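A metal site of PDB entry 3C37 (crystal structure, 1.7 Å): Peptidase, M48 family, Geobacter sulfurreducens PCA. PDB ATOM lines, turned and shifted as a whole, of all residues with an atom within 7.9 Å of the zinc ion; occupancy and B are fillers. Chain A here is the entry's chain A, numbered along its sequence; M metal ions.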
ATOM      1  N   ALA A  76      24.235 -20.214 -15.409  1.00  0.00           N
ATOM      2  CA  ALA A  76      24.785 -21.571 -15.500  1.00  0.00           C
ATOM      3  C   ALA A  76      26.205 -21.387 -16.024  1.00  0.00           C
ATOM      4  O   ALA A  76      26.470 -20.462 -16.787  1.00  0.00           O
ATOM      5  CB  ALA A  76      23.996 -22.441 -16.462  1.00  0.00           C
ATOM      6  N   VAL A 103      20.127 -22.834 -22.747  1.00  0.00           N
ATOM      7  CA  VAL A 103      21.207 -22.327 -21.900  1.00  0.00           C
ATOM      8  C   VAL A 103      22.198 -23.443 -21.597  1.00  0.00           C
ATOM      9  O   VAL A 103      23.398 -23.255 -21.753  1.00  0.00           O
ATOM     10  CB  VAL A 103      20.687 -21.740 -20.577  1.00  0.00           C
ATOM     11  CG1 VAL A 103      21.861 -21.423 -19.636  1.00  0.00           C
ATOM     12  CG2 VAL A 103      19.871 -20.508 -20.858  1.00  0.00           C
ATOM     13  N   HIS A 106      24.490 -24.417 -24.593  1.00  0.00           N
ATOM     14  CA  HIS A 106      25.586 -23.474 -24.815  1.00  0.00           C
ATOM     15  C   HIS A 106      26.744 -23.804 -23.836  1.00  0.00           C
ATOM     16  O   HIS A 106      27.912 -23.900 -24.238  1.00  0.00           O
ATOM     17  CB  HIS A 106      25.027 -22.072 -24.575  1.00  0.00           C
ATOM     18  CG  HIS A 106      26.036 -20.997 -24.806  1.00  0.00           C
ATOM     19  ND1 HIS A 106      26.260 -20.446 -26.052  1.00  0.00           N
ATOM     20  CD2 HIS A 106      26.857 -20.345 -23.953  1.00  0.00           C
ATOM     21  CE1 HIS A 106      27.186 -19.509 -25.948  1.00  0.00           C
ATOM     22  NE2 HIS A 106      27.597 -19.456 -24.695  1.00  0.00           N
ATOM     23  N   GLU A 107      26.431 -23.975 -22.558  1.00  0.00           N
ATOM     24  CA  GLU A 107      27.472 -24.245 -21.532  1.00  0.00           C
ATOM     25  C   GLU A 107      28.157 -25.589 -21.720  1.00  0.00           C
ATOM     26  O   GLU A 107      29.369 -25.715 -21.566  1.00  0.00           O
ATOM     27  CB  GLU A 107      26.874 -24.202 -20.120  1.00  0.00           C
ATOM     28  CG  GLU A 107      26.771 -22.823 -19.580  1.00  0.00           C
ATOM     29  CD  GLU A 107      28.040 -22.006 -19.793  1.00  0.00           C
ATOM     30  OE1 GLU A 107      29.142 -22.350 -19.326  1.00  0.00           O
ATOM     31  OE2 GLU A 107      27.906 -21.005 -20.462  1.00  0.00           O
ATOM     32  N   ASN A 109      28.628 -26.950 -24.466  1.00  0.00           N
ATOM     33  CA  ASN A 109      29.569 -26.816 -25.575  1.00  0.00           C
ATOM     34  C   ASN A 109      30.820 -26.003 -25.301  1.00  0.00           C
ATOM     35  O   ASN A 109      31.862 -26.280 -25.903  1.00  0.00           O
ATOM     36  CB  ASN A 109      28.848 -26.503 -26.876  1.00  0.00           C
ATOM     37  CG  ASN A 109      28.205 -27.745 -27.436  1.00  0.00           C
ATOM     38  OD1 ASN A 109      28.916 -28.679 -27.820  1.00  0.00           O
ATOM     39  ND2 ASN A 109      26.878 -27.781 -27.480  1.00  0.00           N
ATOM     40  N   HIS A 110      30.739 -25.057 -24.374  1.00  0.00           N
ATOM     41  CA  HIS A 110      31.992 -24.509 -23.831  1.00  0.00           C
ATOM     42  C   HIS A 110      32.863 -25.643 -23.246  1.00  0.00           C
ATOM     43  O   HIS A 110      34.093 -25.629 -23.396  1.00  0.00           O
ATOM     44  CB  HIS A 110      31.666 -23.476 -22.745  1.00  0.00           C
ATOM     45  CG  HIS A 110      31.273 -22.125 -23.262  1.00  0.00           C
ATOM     46  ND1 HIS A 110      31.933 -21.485 -24.308  1.00  0.00           N
ATOM     47  CD2 HIS A 110      30.323 -21.267 -22.836  1.00  0.00           C
ATOM     48  CE1 HIS A 110      31.371 -20.308 -24.507  1.00  0.00           C
ATOM     49  NE2 HIS A 110      30.398 -20.152 -23.631  1.00  0.00           N
ATOM     50  N   HIS A 115      36.772 -24.581 -23.766  1.00  0.00           N
ATOM     51  CA  HIS A 115      36.998 -23.127 -23.834  1.00  0.00           C
ATOM     52  C   HIS A 115      37.626 -22.529 -22.567  1.00  0.00           C
ATOM     53  O   HIS A 115      38.448 -21.600 -22.640  1.00  0.00           O
ATOM     54  CB  HIS A 115      35.701 -22.406 -24.163  1.00  0.00           C
ATOM     55  CG  HIS A 115      35.290 -22.568 -25.582  1.00  0.00           C
ATOM     56  ND1 HIS A 115      33.971 -22.484 -25.986  1.00  0.00           N
ATOM     57  CD2 HIS A 115      36.012 -22.853 -26.696  1.00  0.00           C
ATOM     58  CE1 HIS A 115      33.908 -22.667 -27.291  1.00  0.00           C
ATOM     59  NE2 HIS A 115      35.131 -22.897 -27.753  1.00  0.00           N
ATOM     60  N   SER A 156      35.447 -14.700 -19.046  1.00  0.00           N
ATOM     61  CA  SER A 156      34.878 -14.116 -20.259  1.00  0.00           C
ATOM     62  C   SER A 156      35.507 -14.746 -21.496  1.00  0.00           C
ATOM     63  O   SER A 156      36.723 -14.866 -21.604  1.00  0.00           O
ATOM     64  CB  SER A 156      35.036 -12.597 -20.275  1.00  0.00           C
ATOM     65  OG  SER A 156      34.177 -12.021 -21.254  1.00  0.00           O
ATOM     66  N   TYR A 157      34.650 -15.156 -22.420  1.00  0.00           N
ATOM     67  CA  TYR A 157      35.086 -15.879 -23.599  1.00  0.00           C
ATOM     68  C   TYR A 157      35.193 -14.952 -24.794  1.00  0.00           C
ATOM     69  O   TYR A 157      34.376 -14.061 -24.979  1.00  0.00           O
ATOM     70  CB  TYR A 157      34.105 -17.009 -23.935  1.00  0.00           C
ATOM     71  CG  TYR A 157      34.021 -18.077 -22.875  1.00  0.00           C
ATOM     72  CD1 TYR A 157      35.104 -18.899 -22.619  1.00  0.00           C
ATOM     73  CD2 TYR A 157      32.875 -18.262 -22.125  1.00  0.00           C
ATOM     74  CE1 TYR A 157      35.052 -19.886 -21.660  1.00  0.00           C
ATOM     75  CE2 TYR A 157      32.803 -19.261 -21.158  1.00  0.00           C
ATOM     76  CZ  TYR A 157      33.897 -20.063 -20.949  1.00  0.00           C
ATOM     77  OH  TYR A 157      33.845 -21.050 -19.990  1.00  0.00           O
ATOM     78  N   SER A 158      36.194 -15.208 -25.623  1.00  0.00           N
ATOM     79  CA  SER A 158      36.386 -14.479 -26.860  1.00  0.00           C
ATOM     80  C   SER A 158      35.148 -14.606 -27.726  1.00  0.00           C
ATOM     81  O   SER A 158      34.342 -15.542 -27.584  1.00  0.00           O
ATOM     82  CB  SER A 158      37.584 -15.047 -27.622  1.00  0.00           C
ATOM     83  OG  SER A 158      37.276 -16.336 -28.130  1.00  0.00           O
ATOM     84  N   TYR A 161      35.013 -18.033 -29.394  1.00  0.00           N
ATOM     85  CA  TYR A 161      34.547 -19.143 -28.553  1.00  0.00           C
ATOM     86  C   TYR A 161      33.033 -19.066 -28.365  1.00  0.00           C
ATOM     87  O   TYR A 161      32.360 -20.095 -28.371  1.00  0.00           O
ATOM     88  CB  TYR A 161      35.289 -19.156 -27.221  1.00  0.00           C
ATOM     89  CG  TYR A 161      36.764 -19.531 -27.349  1.00  0.00           C
ATOM     90  CD1 TYR A 161      37.291 -20.011 -28.542  1.00  0.00           C
ATOM     91  CD2 TYR A 161      37.608 -19.435 -26.256  1.00  0.00           C
ATOM     92  CE1 TYR A 161      38.641 -20.377 -28.656  1.00  0.00           C
ATOM     93  CE2 TYR A 161      38.956 -19.797 -26.356  1.00  0.00           C
ATOM     94  CZ  TYR A 161      39.460 -20.242 -27.566  1.00  0.00           C
ATOM     95  OH  TYR A 161      40.800 -20.599 -27.668  1.00  0.00           O
ATOM     96  N   GLU A 162      32.510 -17.850 -28.175  1.00  0.00           N
ATOM     97  CA  GLU A 162      31.058 -17.661 -28.092  1.00  0.00           C
ATOM     98  C   GLU A 162      30.359 -18.150 -29.346  1.00  0.00           C
ATOM     99  O   GLU A 162      29.331 -18.841 -29.274  1.00  0.00           O
ATOM    100  CB  GLU A 162      30.708 -16.204 -27.871  1.00  0.00           C
ATOM    101  CG  GLU A 162      30.930 -15.759 -26.468  1.00  0.00           C
ATOM    102  CD  GLU A 162      29.964 -16.426 -25.529  1.00  0.00           C
ATOM    103  OE1 GLU A 162      28.800 -15.994 -25.403  1.00  0.00           O
ATOM    104  OE2 GLU A 162      30.369 -17.408 -24.931  1.00  0.00           O
ATOM    105  N   ASN A 163      30.924 -17.811 -30.503  1.00  0.00           N
ATOM    106  CA  ASN A 163      30.333 -18.256 -31.763  1.00  0.00           C
ATOM    107  C   ASN A 163      30.374 -19.763 -31.874  1.00  0.00           C
ATOM    108  O   ASN A 163      29.424 -20.373 -32.364  1.00  0.00           O
ATOM    109  CB  ASN A 163      31.056 -17.654 -32.975  1.00  0.00           C
ATOM    110  CG  ASN A 163      30.792 -16.159 -33.147  1.00  0.00           C
ATOM    111  OD1 ASN A 163      29.813 -15.608 -32.620  1.00  0.00           O
ATOM    112  ND2 ASN A 163      31.663 -15.495 -33.935  1.00  0.00           N
ATOM    113  N   ALA A 165      30.446 -21.995 -29.357  1.00  0.00           N
ATOM    114  CA  ALA A 165      29.485 -22.521 -28.397  1.00  0.00           C
ATOM    115  C   ALA A 165      28.043 -22.350 -28.920  1.00  0.00           C
ATOM    116  O   ALA A 165      27.186 -23.219 -28.704  1.00  0.00           O
ATOM    117  CB  ALA A 165      29.665 -21.852 -27.040  1.00  0.00           C
ATOM    118  N   ASP A 166      27.771 -21.218 -29.588  1.00  0.00           N
ATOM    119  CA  ASP A 166      26.450 -20.989 -30.191  1.00  0.00           C
ATOM    120  C   ASP A 166      26.172 -21.986 -31.305  1.00  0.00           C
ATOM    121  O   ASP A 166      25.097 -22.602 -31.356  1.00  0.00           O
ATOM    122  CB  ASP A 166      26.377 -19.589 -30.773  1.00  0.00           C
ATOM    123  CG  ASP A 166      26.013 -18.542 -29.738  1.00  0.00           C
ATOM    124  OD1 ASP A 166      25.528 -18.888 -28.643  1.00  0.00           O
ATOM    125  OD2 ASP A 166      26.196 -17.348 -30.044  1.00  0.00           O
ATOM    126  N   LEU A 183      17.510 -20.956 -26.733  1.00  0.00           N
ATOM    127  CA  LEU A 183      18.365 -19.965 -26.074  1.00  0.00           C
ATOM    128  C   LEU A 183      17.907 -18.531 -26.362  1.00  0.00           C
ATOM    129  O   LEU A 183      17.774 -17.721 -25.439  1.00  0.00           O
ATOM    130  CB  LEU A 183      19.838 -20.116 -26.469  1.00  0.00           C
ATOM    131  CG  LEU A 183      20.847 -19.224 -25.706  1.00  0.00           C
ATOM    132  CD1 LEU A 183      20.635 -19.245 -24.196  1.00  0.00           C
ATOM    133  CD2 LEU A 183      22.261 -19.672 -26.050  1.00  0.00           C
ATOM    134  N   THR A 207      28.970 -13.675 -17.925  1.00  0.00           N
ATOM    135  CA  THR A 207      28.992 -12.746 -19.049  1.00  0.00           C
ATOM    136  C   THR A 207      29.184 -13.490 -20.387  1.00  0.00           C
ATOM    137  O   THR A 207      30.306 -13.762 -20.814  1.00  0.00           O
ATOM    138  CB  THR A 207      30.069 -11.628 -18.860  1.00  0.00           C
ATOM    139  OG1 THR A 207      29.721 -10.794 -17.747  1.00  0.00           O
ATOM    140  CG2 THR A 207      30.215 -10.760 -20.118  1.00  0.00           C
ATOM    141  N   HIS A 208      28.056 -13.828 -21.021  1.00  0.00           N
ATOM    142  CA  HIS A 208      28.029 -14.349 -22.387  1.00  0.00           C
ATOM    143  C   HIS A 208      27.217 -13.340 -23.180  1.00  0.00           C
ATOM    144  O   HIS A 208      26.015 -13.534 -23.387  1.00  0.00           O
ATOM    145  CB  HIS A 208      27.351 -15.722 -22.443  1.00  0.00           C
ATOM    146  CG  HIS A 208      27.957 -16.738 -21.525  1.00  0.00           C
ATOM    147  ND1 HIS A 208      28.846 -17.686 -21.960  1.00  0.00           N
ATOM    148  CD2 HIS A 208      27.781 -16.957 -20.200  1.00  0.00           C
ATOM    149  CE1 HIS A 208      29.212 -18.436 -20.929  1.00  0.00           C
ATOM    150  NE2 HIS A 208      28.577 -18.009 -19.851  1.00  0.00           N
ATOM    151  N   PRO A 209      27.871 -12.268 -23.658  1.00  0.00           N
ATOM    152  CA  PRO A 209      27.163 -11.115 -24.245  1.00  0.00           C
ATOM    153  C   PRO A 209      26.368 -11.521 -25.491  1.00  0.00           C
ATOM    154  O   PRO A 209      26.966 -12.044 -26.428  1.00  0.00           O
ATOM    155  CB  PRO A 209      28.300 -10.178 -24.665  1.00  0.00           C
ATOM    156  CG  PRO A 209      29.510 -10.617 -23.875  1.00  0.00           C
ATOM    157  CD  PRO A 209      29.332 -12.108 -23.699  1.00  0.00           C
ATOM    158  N   ARG A 214      25.842 -12.478 -32.692  1.00  0.00           N
ATOM    159  CA  ARG A 214      25.407 -13.773 -32.186  1.00  0.00           C
ATOM    160  C   ARG A 214      23.965 -14.080 -32.590  1.00  0.00           C
ATOM    161  O   ARG A 214      23.668 -15.203 -32.995  1.00  0.00           O
ATOM    162  CB  ARG A 214      25.604 -13.891 -30.663  1.00  0.00           C
ATOM    163  CG  ARG A 214      27.062 -14.164 -30.255  1.00  0.00           C
ATOM    164  CD  ARG A 214      27.195 -14.446 -28.746  1.00  0.00           C
ATOM    165  NE  ARG A 214      26.492 -15.646 -28.267  1.00  0.00           N
ATOM    166  CZ  ARG A 214      25.995 -15.790 -27.036  1.00  0.00           C
ATOM    167  NH1 ARG A 214      26.111 -14.802 -26.156  1.00  0.00           N
ATOM    168  NH2 ARG A 214      25.368 -16.906 -26.684  1.00  0.00           N
HETATM  169 ZN    ZN M   1      29.193 -18.485 -23.808  1.00  0.00          ZN
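The zinc ion is bound by the side-chain carboxylate of Glu 162, a ring nitrogen (ND1) of His 208, a ring nitrogen (NE2) of His 110 and a ring nitrogen (NE2) of His 106.
Within 4 Å of the zinc ion: His 106, His 110, Glu 162 and His 208.
The guanidinium group (NH1) of Arg 214 lies within salt-bridge range of the side-chain carboxylate (OE1) of Glu 162.
NE2 of His 208 sits close to OE2 of Glu 107, at 3.1 Å.
The backbone carbonyl oxygen of His 208 lies within hydrogen-bond range of the guanidinium group of Arg 214 (3.0 Å).
ND1 of His 110 lies within hydrogen-bond range of ND1 of His 115.
OD1 of Asp 166 sits at hydrogen-bond distance from ND1 of His 106, 3.1 Å away.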
